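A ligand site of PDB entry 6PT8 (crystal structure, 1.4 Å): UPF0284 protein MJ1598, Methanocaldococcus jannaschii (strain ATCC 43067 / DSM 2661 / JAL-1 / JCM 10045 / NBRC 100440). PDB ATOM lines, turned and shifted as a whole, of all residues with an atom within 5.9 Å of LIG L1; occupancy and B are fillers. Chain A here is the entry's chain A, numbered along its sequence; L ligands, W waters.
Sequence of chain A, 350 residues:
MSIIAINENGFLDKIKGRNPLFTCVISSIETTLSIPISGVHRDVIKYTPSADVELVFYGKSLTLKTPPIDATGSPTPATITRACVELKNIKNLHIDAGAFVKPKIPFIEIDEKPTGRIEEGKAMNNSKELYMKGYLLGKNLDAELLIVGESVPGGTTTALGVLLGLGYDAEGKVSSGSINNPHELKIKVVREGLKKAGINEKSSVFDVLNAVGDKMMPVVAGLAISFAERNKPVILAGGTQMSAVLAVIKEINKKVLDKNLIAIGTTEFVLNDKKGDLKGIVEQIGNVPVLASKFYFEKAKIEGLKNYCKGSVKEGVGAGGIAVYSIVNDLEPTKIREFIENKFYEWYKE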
ATOM      1  N   ILE A  37     -13.716 -10.133 -10.013  1.00  0.00           N
ATOM      2  CA  ILE A  37     -13.617  -9.024 -10.950  1.00  0.00           C
ATOM      3  C   ILE A  37     -14.886  -8.817 -11.774  1.00  0.00           C
ATOM      4  O   ILE A  37     -15.109  -7.718 -12.277  1.00  0.00           O
ATOM      5  CB  ILE A  37     -12.408  -9.179 -11.903  1.00  0.00           C
ATOM      6  CG1 ILE A  37     -12.364 -10.564 -12.574  1.00  0.00           C
ATOM      7  CG2 ILE A  37     -11.104  -8.883 -11.149  1.00  0.00           C
ATOM      8  CD1 ILE A  37     -11.367 -10.663 -13.758  1.00  0.00           C
ATOM      9  N   SER A  38     -15.723  -9.841 -11.935  1.00  0.00           N
ATOM     10  CA  SER A  38     -16.880  -9.788 -12.834  1.00  0.00           C
ATOM     11  C   SER A  38     -18.144  -9.366 -12.101  1.00  0.00           C
ATOM     12  O   SER A  38     -18.385  -9.767 -10.953  1.00  0.00           O
ATOM     13  CB  SER A  38     -17.115 -11.163 -13.466  1.00  0.00           C
ATOM     14  OG  SER A  38     -18.312 -11.175 -14.222  1.00  0.00           O
ATOM     15  N   GLY A  39     -19.006  -8.652 -12.811  1.00  0.00           N
ATOM     16  CA  GLY A  39     -20.336  -8.324 -12.337  1.00  0.00           C
ATOM     17  C   GLY A  39     -21.372  -9.389 -12.565  1.00  0.00           C
ATOM     18  O   GLY A  39     -22.517  -9.205 -12.169  1.00  0.00           O
ATOM     19  N   VAL A  40     -21.024 -10.486 -13.243  1.00  0.00           N
ATOM     20  CA  VAL A  40     -21.930 -11.617 -13.391  1.00  0.00           C
ATOM     21  C   VAL A  40     -21.993 -12.372 -12.085  1.00  0.00           C
ATOM     22  O   VAL A  40     -20.974 -12.574 -11.420  1.00  0.00           O
ATOM     23  CB  VAL A  40     -21.462 -12.512 -14.547  1.00  0.00           C
ATOM     24  CG1 VAL A  40     -22.362 -13.714 -14.650  1.00  0.00           C
ATOM     25  CG2 VAL A  40     -21.489 -11.770 -15.877  1.00  0.00           C
ATOM     26  N   HIS A  41     -23.186 -12.817 -11.697  1.00  0.00           N
ATOM     27  CA  HIS A  41     -23.335 -13.466 -10.398  1.00  0.00           C
ATOM     28  C   HIS A  41     -22.446 -14.709 -10.313  1.00  0.00           C
ATOM     29  O   HIS A  41     -22.407 -15.530 -11.231  1.00  0.00           O
ATOM     30  CB  HIS A  41     -24.787 -13.859 -10.146  1.00  0.00           C
ATOM     31  CG  HIS A  41     -25.093 -14.091  -8.712  1.00  0.00           C
ATOM     32  ND1 HIS A  41     -24.624 -15.188  -8.026  1.00  0.00           N
ATOM     33  CD2 HIS A  41     -25.801 -13.357  -7.820  1.00  0.00           C
ATOM     34  CE1 HIS A  41     -25.021 -15.117  -6.763  1.00  0.00           C
ATOM     35  NE2 HIS A  41     -25.749 -14.025  -6.616  1.00  0.00           N
ATOM     36  N   ILE A  45     -21.678 -17.715 -13.174  1.00  0.00           N
ATOM     37  CA  ILE A  45     -20.681 -17.166 -14.101  1.00  0.00           C
ATOM     38  C   ILE A  45     -20.093 -18.228 -15.020  1.00  0.00           C
ATOM     39  O   ILE A  45     -19.856 -17.973 -16.211  1.00  0.00           O
ATOM     40  CB  ILE A  45     -19.600 -16.390 -13.329  1.00  0.00           C
ATOM     41  CG1 ILE A  45     -18.723 -15.617 -14.313  1.00  0.00           C
ATOM     42  CG2 ILE A  45     -18.775 -17.307 -12.456  1.00  0.00           C
ATOM     43  CD1 ILE A  45     -17.859 -14.611 -13.613  1.00  0.00           C
ATOM     44  N   THR A  48     -22.590 -18.858 -17.861  1.00  0.00           N
ATOM     45  CA  THR A  48     -23.275 -17.675 -18.411  1.00  0.00           C
ATOM     46  C   THR A  48     -23.042 -17.525 -19.899  1.00  0.00           C
ATOM     47  O   THR A  48     -24.031 -17.285 -20.616  1.00  0.00           O
ATOM     48  CB  THR A  48     -22.860 -16.455 -17.595  1.00  0.00           C
ATOM     49  OG1 THR A  48     -23.558 -16.494 -16.336  1.00  0.00           O
ATOM     50  CG2 THR A  48     -23.203 -15.111 -18.316  1.00  0.00           C
ATOM     51  N   ASP A  52     -26.318 -17.689 -22.305  1.00  0.00           N
ATOM     52  CA  ASP A  52     -26.685 -16.485 -23.033  1.00  0.00           C
ATOM     53  C   ASP A  52     -26.985 -16.811 -24.492  1.00  0.00           C
ATOM     54  O   ASP A  52     -28.002 -16.377 -25.030  1.00  0.00           O
ATOM     55  CB  ASP A  52     -25.547 -15.455 -22.954  1.00  0.00           C
ATOM     56  CG  ASP A  52     -25.507 -14.682 -21.644  1.00  0.00           C
ATOM     57  OD1 ASP A  52     -26.538 -14.629 -20.927  1.00  0.00           O
ATOM     58  OD2 ASP A  52     -24.444 -14.064 -21.358  1.00  0.00           O
ATOM     59  N   PRO A  68     -29.011 -16.246 -17.218  1.00  0.00           N
ATOM     60  CA  PRO A  68     -28.096 -15.677 -16.222  1.00  0.00           C
ATOM     61  C   PRO A  68     -28.580 -14.360 -15.618  1.00  0.00           C
ATOM     62  O   PRO A  68     -29.496 -13.711 -16.119  1.00  0.00           O
ATOM     63  CB  PRO A  68     -26.781 -15.467 -17.010  1.00  0.00           C
ATOM     64  CG  PRO A  68     -26.863 -16.487 -18.083  1.00  0.00           C
ATOM     65  CD  PRO A  68     -28.312 -16.523 -18.488  1.00  0.00           C
ATOM     66  N   ILE A  69     -27.896 -13.972 -14.533  1.00  0.00           N
ATOM     67  CA  ILE A  69     -28.185 -12.752 -13.788  1.00  0.00           C
ATOM     68  C   ILE A  69     -26.854 -12.109 -13.403  1.00  0.00           C
ATOM     69  O   ILE A  69     -25.836 -12.774 -13.258  1.00  0.00           O
ATOM     70  CB  ILE A  69     -29.039 -13.016 -12.534  1.00  0.00           C
ATOM     71  CG1 ILE A  69     -28.389 -14.051 -11.614  1.00  0.00           C
ATOM     72  CG2 ILE A  69     -30.438 -13.454 -12.970  1.00  0.00           C
ATOM     73  CD1 ILE A  69     -28.964 -14.051 -10.176  1.00  0.00           C
ATOM     74  N   ASP A  70     -26.888 -10.790 -13.183  1.00  0.00           N
ATOM     75  CA  ASP A  70     -25.724 -10.097 -12.619  1.00  0.00           C
ATOM     76  C   ASP A  70     -25.734 -10.183 -11.096  1.00  0.00           C
ATOM     77  O   ASP A  70     -26.594 -10.834 -10.479  1.00  0.00           O
ATOM     78  CB  ASP A  70     -25.646  -8.665 -13.149  1.00  0.00           C
ATOM     79  CG  ASP A  70     -26.462  -7.665 -12.326  1.00  0.00           C
ATOM     80  OD1 ASP A  70     -27.420  -8.077 -11.651  1.00  0.00           O
ATOM     81  OD2 ASP A  70     -26.134  -6.453 -12.388  1.00  0.00           O
ATOM     82  N   SER A  74     -30.252  -8.890 -11.572  1.00  0.00           N
ATOM     83  CA  SER A  74     -30.893  -8.394 -12.789  1.00  0.00           C
ATOM     84  C   SER A  74     -30.663  -9.345 -13.963  1.00  0.00           C
ATOM     85  O   SER A  74     -29.639 -10.032 -14.024  1.00  0.00           O
ATOM     86  CB  SER A  74     -30.368  -7.030 -13.137  1.00  0.00           C
ATOM     87  OG  SER A  74     -30.800  -6.068 -12.185  1.00  0.00           O
ATOM     88  N   PRO A  75     -31.601  -9.387 -14.905  1.00  0.00           N
ATOM     89  CA  PRO A  75     -31.528 -10.386 -15.989  1.00  0.00           C
ATOM     90  C   PRO A  75     -30.457 -10.071 -17.032  1.00  0.00           C
ATOM     91  O   PRO A  75     -30.170  -8.916 -17.350  1.00  0.00           O
ATOM     92  CB  PRO A  75     -32.914 -10.312 -16.626  1.00  0.00           C
ATOM     93  CG  PRO A  75     -33.340  -8.868 -16.397  1.00  0.00           C
ATOM     94  CD  PRO A  75     -32.815  -8.567 -15.020  1.00  0.00           C
ATOM     95  N   THR A  76     -29.928 -11.147 -17.580  1.00  0.00           N
ATOM     96  CA  THR A  76     -28.912 -11.091 -18.627  1.00  0.00           C
ATOM     97  C   THR A  76     -29.349 -10.166 -19.762  1.00  0.00           C
ATOM     98  O   THR A  76     -30.532 -10.159 -20.158  1.00  0.00           O
ATOM     99  CB  THR A  76     -28.692 -12.487 -19.217  1.00  0.00           C
ATOM    100  OG1 THR A  76     -27.791 -12.328 -20.339  1.00  0.00           O
ATOM    101  CG2 THR A  76     -29.998 -13.133 -19.704  1.00  0.00           C
ATOM    102  N   PRO A  77     -28.412  -9.444 -20.381  1.00  0.00           N
ATOM    103  CA  PRO A  77     -28.760  -8.654 -21.569  1.00  0.00           C
ATOM    104  C   PRO A  77     -29.062  -9.513 -22.782  1.00  0.00           C
ATOM    105  O   PRO A  77     -29.529  -8.970 -23.787  1.00  0.00           O
ATOM    106  CB  PRO A  77     -27.532  -7.778 -21.769  1.00  0.00           C
ATOM    107  CG  PRO A  77     -26.381  -8.649 -21.250  1.00  0.00           C
ATOM    108  CD  PRO A  77     -26.954  -9.437 -20.091  1.00  0.00           C
ATOM    109  N   ALA A  78     -28.844 -10.814 -22.706  1.00  0.00           N
ATOM    110  CA  ALA A  78     -29.362 -11.698 -23.746  1.00  0.00           C
ATOM    111  C   ALA A  78     -30.863 -11.595 -23.883  1.00  0.00           C
ATOM    112  O   ALA A  78     -31.398 -11.982 -24.920  1.00  0.00           O
ATOM    113  CB  ALA A  78     -28.932 -13.137 -23.489  1.00  0.00           C
ATOM    114  N   GLU A 150     -20.373 -10.120 -27.805  1.00  0.00           N
ATOM    115  CA  GLU A 150     -19.560 -10.978 -26.958  1.00  0.00           C
ATOM    116  C   GLU A 150     -20.353 -11.399 -25.734  1.00  0.00           C
ATOM    117  O   GLU A 150     -21.287 -10.708 -25.292  1.00  0.00           O
ATOM    118  CB  GLU A 150     -18.288 -10.277 -26.461  1.00  0.00           C
ATOM    119  CG  GLU A 150     -18.512  -8.937 -25.746  1.00  0.00           C
ATOM    120  CD  GLU A 150     -19.157  -9.033 -24.345  1.00  0.00           C
ATOM    121  OE1 GLU A 150     -20.088  -8.231 -24.047  1.00  0.00           O
ATOM    122  OE2 GLU A 150     -18.705  -9.875 -23.532  1.00  0.00           O
ATOM    123  N   SER A 151     -19.940 -12.523 -25.136  1.00  0.00           N
ATOM    124  CA  SER A 151     -20.326 -12.795 -23.754  1.00  0.00           C
ATOM    125  C   SER A 151     -19.084 -13.362 -23.070  1.00  0.00           C
ATOM    126  O   SER A 151     -18.785 -14.543 -23.239  1.00  0.00           O
ATOM    127  CB  SER A 151     -21.526 -13.697 -23.598  1.00  0.00           C
ATOM    128  OG  SER A 151     -21.880 -13.691 -22.191  1.00  0.00           O
ATOM    129  N   VAL A 152     -18.376 -12.519 -22.318  1.00  0.00           N
ATOM    130  CA  VAL A 152     -17.132 -12.866 -21.658  1.00  0.00           C
ATOM    131  C   VAL A 152     -17.155 -12.278 -20.249  1.00  0.00           C
ATOM    132  O   VAL A 152     -16.791 -11.105 -20.043  1.00  0.00           O
ATOM    133  CB  VAL A 152     -15.908 -12.339 -22.424  1.00  0.00           C
ATOM    134  CG1 VAL A 152     -14.659 -12.836 -21.736  1.00  0.00           C
ATOM    135  CG2 VAL A 152     -15.918 -12.766 -23.893  1.00  0.00           C
ATOM    136  N   PRO A 153     -17.614 -13.039 -19.259  1.00  0.00           N
ATOM    137  CA  PRO A 153     -17.560 -12.527 -17.886  1.00  0.00           C
ATOM    138  C   PRO A 153     -16.115 -12.306 -17.480  1.00  0.00           C
ATOM    139  O   PRO A 153     -15.258 -13.156 -17.686  1.00  0.00           O
ATOM    140  CB  PRO A 153     -18.263 -13.618 -17.083  1.00  0.00           C
ATOM    141  CG  PRO A 153     -19.120 -14.338 -18.086  1.00  0.00           C
ATOM    142  CD  PRO A 153     -18.333 -14.330 -19.353  1.00  0.00           C
ATOM    143  N   GLY A 154     -15.862 -11.115 -16.916  1.00  0.00           N
ATOM    144  CA  GLY A 154     -14.494 -10.664 -16.680  1.00  0.00           C
ATOM    145  C   GLY A 154     -13.914  -9.860 -17.816  1.00  0.00           C
ATOM    146  O   GLY A 154     -12.812  -9.301 -17.679  1.00  0.00           O
ATOM    147  N   GLY A 155     -14.666  -9.704 -18.905  1.00  0.00           N
ATOM    148  CA  GLY A 155     -14.140  -9.039 -20.081  1.00  0.00           C
ATOM    149  C   GLY A 155     -13.856  -7.554 -19.931  1.00  0.00           C
ATOM    150  O   GLY A 155     -13.055  -7.022 -20.688  1.00  0.00           O
ATOM    151  N   THR A 156     -14.479  -6.875 -18.977  1.00  0.00           N
ATOM    152  CA  THR A 156     -14.075  -5.480 -18.772  1.00  0.00           C
ATOM    153  C   THR A 156     -12.688  -5.386 -18.148  1.00  0.00           C
ATOM    154  O   THR A 156     -12.000  -4.371 -18.354  1.00  0.00           O
ATOM    155  CB  THR A 156     -15.093  -4.639 -17.990  1.00  0.00           C
ATOM    156  OG1 THR A 156     -15.281  -5.125 -16.654  1.00  0.00           O
ATOM    157  CG2 THR A 156     -16.453  -4.593 -18.714  1.00  0.00           C
ATOM    158  N   THR A 157     -12.242  -6.420 -17.453  1.00  0.00           N
ATOM    159  CA  THR A 157     -10.891  -6.443 -16.891  1.00  0.00           C
ATOM    160  C   THR A 157      -9.848  -6.705 -17.965  1.00  0.00           C
ATOM    161  O   THR A 157      -8.818  -6.002 -18.032  1.00  0.00           O
ATOM    162  CB  THR A 157     -10.803  -7.479 -15.782  1.00  0.00           C
ATOM    163  OG1 THR A 157     -11.746  -7.142 -14.745  1.00  0.00           O
ATOM    164  CG2 THR A 157      -9.420  -7.525 -15.127  1.00  0.00           C
ATOM    165  N   SER A 175     -15.998  -0.155 -18.065  1.00  0.00           N
ATOM    166  CA  SER A 175     -17.297  -0.269 -17.406  1.00  0.00           C
ATOM    167  C   SER A 175     -17.334  -1.540 -16.574  1.00  0.00           C
ATOM    168  O   SER A 175     -16.296  -2.076 -16.161  1.00  0.00           O
ATOM    169  CB  SER A 175     -18.403  -0.132 -18.455  1.00  0.00           C
ATOM    170  OG  SER A 175     -19.703  -0.137 -17.876  1.00  0.00           O
ATOM    171  N   SER A 176     -18.528  -2.023 -16.259  1.00  0.00           N
ATOM    172  CA  SER A 176     -18.657  -3.202 -15.415  1.00  0.00           C
ATOM    173  C   SER A 176     -20.044  -3.775 -15.643  1.00  0.00           C
ATOM    174  O   SER A 176     -21.004  -3.044 -15.904  1.00  0.00           O
ATOM    175  CB  SER A 176     -18.494  -2.873 -13.922  1.00  0.00           C
ATOM    176  OG  SER A 176     -19.458  -1.933 -13.521  1.00  0.00           O
ATOM    177  N   GLY A 177     -20.135  -5.085 -15.515  1.00  0.00           N
ATOM    178  CA  GLY A 177     -21.409  -5.751 -15.718  1.00  0.00           C
ATOM    179  C   GLY A 177     -22.378  -5.690 -14.571  1.00  0.00           C
ATOM    180  O   GLY A 177     -23.411  -6.372 -14.605  1.00  0.00           O
ATOM    181  N   SER A 178     -22.064  -4.924 -13.519  1.00  0.00           N
ATOM    182  CA  SER A 178     -23.013  -4.689 -12.431  1.00  0.00           C
ATOM    183  C   SER A 178     -22.728  -3.322 -11.845  1.00  0.00           C
ATOM    184  O   SER A 178     -21.889  -2.569 -12.338  1.00  0.00           O
ATOM    185  CB  SER A 178     -22.966  -5.789 -11.380  1.00  0.00           C
ATOM    186  OG  SER A 178     -24.132  -5.753 -10.539  1.00  0.00           O
ATOM    187  N   LYS A 186      -9.356  -4.508 -10.419  1.00  0.00           N
ATOM    188  CA  LYS A 186      -9.066  -4.729 -11.839  1.00  0.00           C
ATOM    189  C   LYS A 186      -7.668  -4.254 -12.206  1.00  0.00           C
ATOM    190  O   LYS A 186      -6.949  -4.937 -12.952  1.00  0.00           O
ATOM    191  CB  LYS A 186     -10.102  -4.048 -12.726  1.00  0.00           C
ATOM    192  CG  LYS A 186     -11.486  -4.603 -12.634  1.00  0.00           C
ATOM    193  CD  LYS A 186     -12.455  -3.908 -13.587  1.00  0.00           C
ATOM    194  CE  LYS A 186     -13.793  -4.575 -13.480  1.00  0.00           C
ATOM    195  NZ  LYS A 186     -14.847  -3.858 -14.174  1.00  0.00           N
ATOM    196  N   GLN A 241     -15.492  -3.181 -23.642  1.00  0.00           N
ATOM    197  CA  GLN A 241     -14.817  -4.337 -24.202  1.00  0.00           C
ATOM    198  C   GLN A 241     -14.532  -4.162 -25.698  1.00  0.00           C
ATOM    199  O   GLN A 241     -13.460  -4.532 -26.193  1.00  0.00           O
ATOM    200  CB  GLN A 241     -15.652  -5.599 -23.998  1.00  0.00           C
ATOM    201  CG  GLN A 241     -15.748  -6.021 -22.532  1.00  0.00           C
ATOM    202  CD  GLN A 241     -16.572  -7.254 -22.376  1.00  0.00           C
ATOM    203  OE1 GLN A 241     -17.675  -7.191 -21.818  1.00  0.00           O
ATOM    204  NE2 GLN A 241     -16.078  -8.363 -22.891  1.00  0.00           N
ATOM    205  N   VAL A 313     -26.101  -4.722 -14.958  1.00  0.00           N
ATOM    206  CA  VAL A 313     -25.915  -5.326 -16.294  1.00  0.00           C
ATOM    207  C   VAL A 313     -25.294  -4.397 -17.316  1.00  0.00           C
ATOM    208  O   VAL A 313     -24.165  -4.609 -17.767  1.00  0.00           O
ATOM    209  CB  VAL A 313     -27.215  -5.961 -16.843  1.00  0.00           C
ATOM    210  CG1 VAL A 313     -26.946  -6.559 -18.219  1.00  0.00           C
ATOM    211  CG2 VAL A 313     -27.759  -7.002 -15.887  1.00  0.00           C
ATOM    212  N   LYS A 314     -26.074  -3.405 -17.771  1.00  0.00           N
ATOM    213  CA  LYS A 314     -25.723  -2.361 -18.711  1.00  0.00           C
ATOM    214  C   LYS A 314     -25.681  -2.806 -20.175  1.00  0.00           C
ATOM    215  O   LYS A 314     -26.204  -2.117 -21.048  1.00  0.00           O
ATOM    216  CB  LYS A 314     -24.381  -1.681 -18.415  1.00  0.00           C
ATOM    217  CG  LYS A 314     -24.265  -1.055 -17.041  1.00  0.00           C
ATOM    218  CD  LYS A 314     -22.957  -0.291 -16.939  1.00  0.00           C
ATOM    219  CE  LYS A 314     -22.687   0.238 -15.542  1.00  0.00           C
ATOM    220  NZ  LYS A 314     -22.444  -0.864 -14.570  1.00  0.00           N
ATOM    221  N   GLU A 315     -25.024  -3.932 -20.460  1.00  0.00           N
ATOM    222  CA  GLU A 315     -24.647  -4.313 -21.813  1.00  0.00           C
ATOM    223  C   GLU A 315     -24.231  -5.773 -21.800  1.00  0.00           C
ATOM    224  O   GLU A 315     -23.963  -6.360 -20.747  1.00  0.00           O
ATOM    225  CB  GLU A 315     -23.488  -3.439 -22.313  1.00  0.00           C
ATOM    226  CG  GLU A 315     -22.812  -3.826 -23.634  1.00  0.00           C
ATOM    227  CD  GLU A 315     -23.704  -3.682 -24.819  1.00  0.00           C
ATOM    228  OE1 GLU A 315     -24.543  -4.564 -25.073  1.00  0.00           O
ATOM    229  OE2 GLU A 315     -23.524  -2.670 -25.534  1.00  0.00           O
ATOM    230  N   GLY A 316     -24.223  -6.372 -22.986  1.00  0.00           N
ATOM    231  CA  GLY A 316     -23.633  -7.679 -23.192  1.00  0.00           C
ATOM    232  C   GLY A 316     -24.427  -8.490 -24.200  1.00  0.00           C
ATOM    233  O   GLY A 316     -25.579  -8.190 -24.536  1.00  0.00           O
ATOM    234  N   VAL A 317     -23.799  -9.549 -24.695  1.00  0.00           N
ATOM    235  CA  VAL A 317     -24.420 -10.446 -25.650  1.00  0.00           C
ATOM    236  C   VAL A 317     -24.874  -9.653 -26.885  1.00  0.00           C
ATOM    237  O   VAL A 317     -25.872  -9.982 -27.531  1.00  0.00           O
ATOM    238  CB  VAL A 317     -25.564 -11.263 -25.034  1.00  0.00           C
ATOM    239  CG1 VAL A 317     -25.869 -12.477 -25.907  1.00  0.00           C
ATOM    240  CG2 VAL A 317     -25.204 -11.746 -23.630  1.00  0.00           C
HETATM  241  C1  LIG L   1     -23.128 -11.137 -20.290  1.00  0.00           C
HETATM  242  N1  LIG L   1     -24.055 -11.984 -19.829  1.00  0.00           N
HETATM  243  C2  LIG L   1     -24.487 -11.387 -18.592  1.00  0.00           C
HETATM  244  C3  LIG L   1     -23.770 -10.178 -18.401  1.00  0.00           C
HETATM  245  N2  LIG L   1     -22.928 -10.100 -19.485  1.00  0.00           N
HETATM  246  N3  LIG L   1     -25.383 -11.853 -17.744  1.00  0.00           N
HETATM  247  C4  LIG L   1     -25.636 -11.116 -16.666  1.00  0.00           C
HETATM  248  N4  LIG L   1     -25.004  -9.964 -16.383  1.00  0.00           N
HETATM  249  C5  LIG L   1     -24.079  -9.479 -17.245  1.00  0.00           C
HETATM  250  N5  LIG L   1     -23.410  -8.279 -16.917  1.00  0.00           N
HETATM  251  P1  LIG L   1     -17.782  -7.930 -16.318  1.00  0.00           P
HETATM  252  O1  LIG L   1     -18.194  -7.134 -15.114  1.00  0.00           O
HETATM  253  O2  LIG L   1     -16.437  -7.555 -16.769  1.00  0.00           O
HETATM  254  O3  LIG L   1     -17.848  -9.390 -16.125  1.00  0.00           O
HETATM  255  O4  LIG L   1     -18.885  -7.509 -17.450  1.00  0.00           O
HETATM  256  C6  LIG L   1     -18.850  -8.169 -18.710  1.00  0.00           C
HETATM  257  C7  LIG L   1     -19.871  -9.254 -18.798  1.00  0.00           C
HETATM  258  O5  LIG L   1     -21.222  -8.663 -18.648  1.00  0.00           O
HETATM  259  C8  LIG L   1     -19.905  -9.925 -20.160  1.00  0.00           C
HETATM  260  O6  LIG L   1     -20.247 -11.278 -19.948  1.00  0.00           O
HETATM  261  C9  LIG L   1     -20.963  -9.194 -20.871  1.00  0.00           C
HETATM  262  O7  LIG L   1     -21.461  -9.862 -22.024  1.00  0.00           O
HETATM  263  C10 LIG L   1     -22.028  -9.019 -19.811  1.00  0.00           C
HETATM  264  N1  LG2 L   2     -20.922  -5.887 -20.396  1.00  0.00           N
HETATM  265  C1  LG2 L   2     -19.980  -5.196 -21.066  1.00  0.00           C
HETATM  266  C2  LG2 L   2     -19.680  -3.899 -20.710  1.00  0.00           C
HETATM  267  C3  LG2 L   2     -20.320  -3.291 -19.642  1.00  0.00           C
HETATM  268  C4  LG2 L   2     -21.253  -3.983 -18.975  1.00  0.00           C
HETATM  269  C5  LG2 L   2     -21.548  -5.289 -19.344  1.00  0.00           C
HETATM  270  C6  LG2 L   2     -18.626  -3.151 -21.489  1.00  0.00           C
HETATM  271  O1  LG2 L   2     -18.283  -2.007 -21.116  1.00  0.00           O
HETATM  272  O2  LG2 L   2     -18.100  -3.703 -22.495  1.00  0.00           O
HETATM  273  O   HOH W   1     -16.836  -5.806 -13.278  1.00  0.00           O
HETATM  274  O   HOH W   2     -14.358  -7.922 -14.987  1.00  0.00           O
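OD2 of Asp 52 is in hydrogen-bond range of N1 of LIG L1 (2.6 Å). OG of Ser 38 sits at hydrogen-bond distance from O3 of LIG L1 (2.7 Å). The backbone NH (N) of Thr 156 is in hydrogen-bond range of an oxygen (O2) of LIG L1, at 3.0 Å. The side-chain hydroxyl (OG1) of Thr 156 sits at hydrogen-bond distance from an oxygen (O2) of LIG L1, at 2.7 Å. The backbone NH of Gly 154 is in hydrogen-bond range of an oxygen (O3) of LIG L1, at 2.7 Å. The backbone NH (N) of Gly 177 is in hydrogen-bond range of an oxygen (O1) of LIG L1, 2.9 Å away. O of Gly 177 is in hydrogen-bond range of N5 of LIG L1, 3.0 Å away. N of Gly 39 is in hydrogen-bond range of O1 of LIG L1, 2.9 Å away. O of Glu 150 sits close to O7 of LIG L1, at 3.4 Å. The side-chain carboxylate (OE1) of Glu 150 sits at hydrogen-bond distance from an oxygen (O7) of LIG L1, at 2.9 Å. O6 of LIG L1 sits close to N of Val 152 (3.3 Å). The backbone carbonyl oxygen (O) of Val 152 lies close to an oxygen (O6) of LIG L1, at 3.5 Å. The backbone NH (N) of Gln 241 sits at hydrogen-bond distance from an oxygen (O2) of LG2 L2, at 2.9 Å.
The side-chain hydroxyl (OG1) of Thr 76 lies within hydrogen-bond range of the side-chain carboxylate (OD1) of Asp 52. O of Glu 150 is in hydrogen-bond range of N of Val 317 (2.8 Å). The backbone NH of Val 313 sits at hydrogen-bond distance from the side-chain carboxylate of Asp 70 (3.1 Å). OD1 of Asp 70 lies within hydrogen-bond range of N of Ser 74 (2.9 Å). The backbone carbonyl oxygen (O) of Pro 68 is in hydrogen-bond range of the backbone NH (N) of Thr 76 (3.0 Å). The backbone carbonyl oxygen (O) of Ile 69 sits at hydrogen-bond distance from the backbone NH (N) of His 41. The side-chain hydroxyl (OG) of Ser 176 is in hydrogen-bond range of the backbone carbonyl oxygen (O) of Ser 178. NZ of Lys 314 is in hydrogen-bond range of O of Ser 176 (2.9 Å).
The backbone nitrogen (N) of Pro 153 lies close to an oxygen (O6) of LIG L1 (3.2 Å). CG2 of Val 40 touches C5 of LIG L1 (3.7 Å). Thr 48 touches LIG L1. Pro 68 touches LIG L1. Ile 69 touches LIG L1. CB of Asp 70 touches N4 of LIG L1, at 3.5 Å. Thr 76 touches LIG L1 (OG1 to N3, 3.6 Å). Pro 77 touches LIG L1 (CD to C2, 3.5 Å). OG of Ser 151 touches C1 of LIG L1 (3.4 Å). Gly 155 touches LIG L1. Ser 176 touches LIG L1. Gln 241 touches LIG L1 (OE1 to C6, 3.5 Å). Val 313 touches LIG L1. O of Glu 315 touches C10 of LIG L1 (3.4 Å). CA of Gly 316 touches O7 of LIG L1 (3.3 Å). Val 317 touches LIG L1 (N to O7, 3.6 Å). Hydrophobic or aromatic side chains within 4 Å of LIG L1: Val 40, Pro 68, Pro 77, Pro 153 and Val 317. 24 residues have an atom within 4 Å of LIG L1: Ser 38, Gly 39, Val 40, Thr 48, Asp 52, Pro 68, Ile 69, Asp 70, Thr 76, Pro 77, Glu 150, Ser 151, Val 152, Pro 153, Gly 154, Gly 155, Thr 156, Ser 176, Gly 177, Gln 241, Val 313, Glu 315, Gly 316 and Val 317. Along chain A the residues within 4 Å of LIG L1 span positions 38 to 317. The nearest printed residue that does not touch LIG L1 is Ile 37 (4.2 Å).
Water W1 lies within hydrogen-bond range of an oxygen (O1) of LIG L1 (2.6 Å), the backbone carbonyl oxygen (O) of Ile 37 (2.8 Å) and the side-chain amino group (NZ) of Lys 186 (2.9 Å). Water W2 lies within hydrogen-bond range of the side-chain hydroxyl of Thr 157 (2.7 Å), an oxygen (O2) of LIG L1 (2.8 Å), the backbone carbonyl oxygen of Ile 37 (2.8 Å), the side-chain hydroxyl of Thr 156 (3.4 Å) and the backbone carbonyl oxygen of Gly 154 (3.4 Å).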
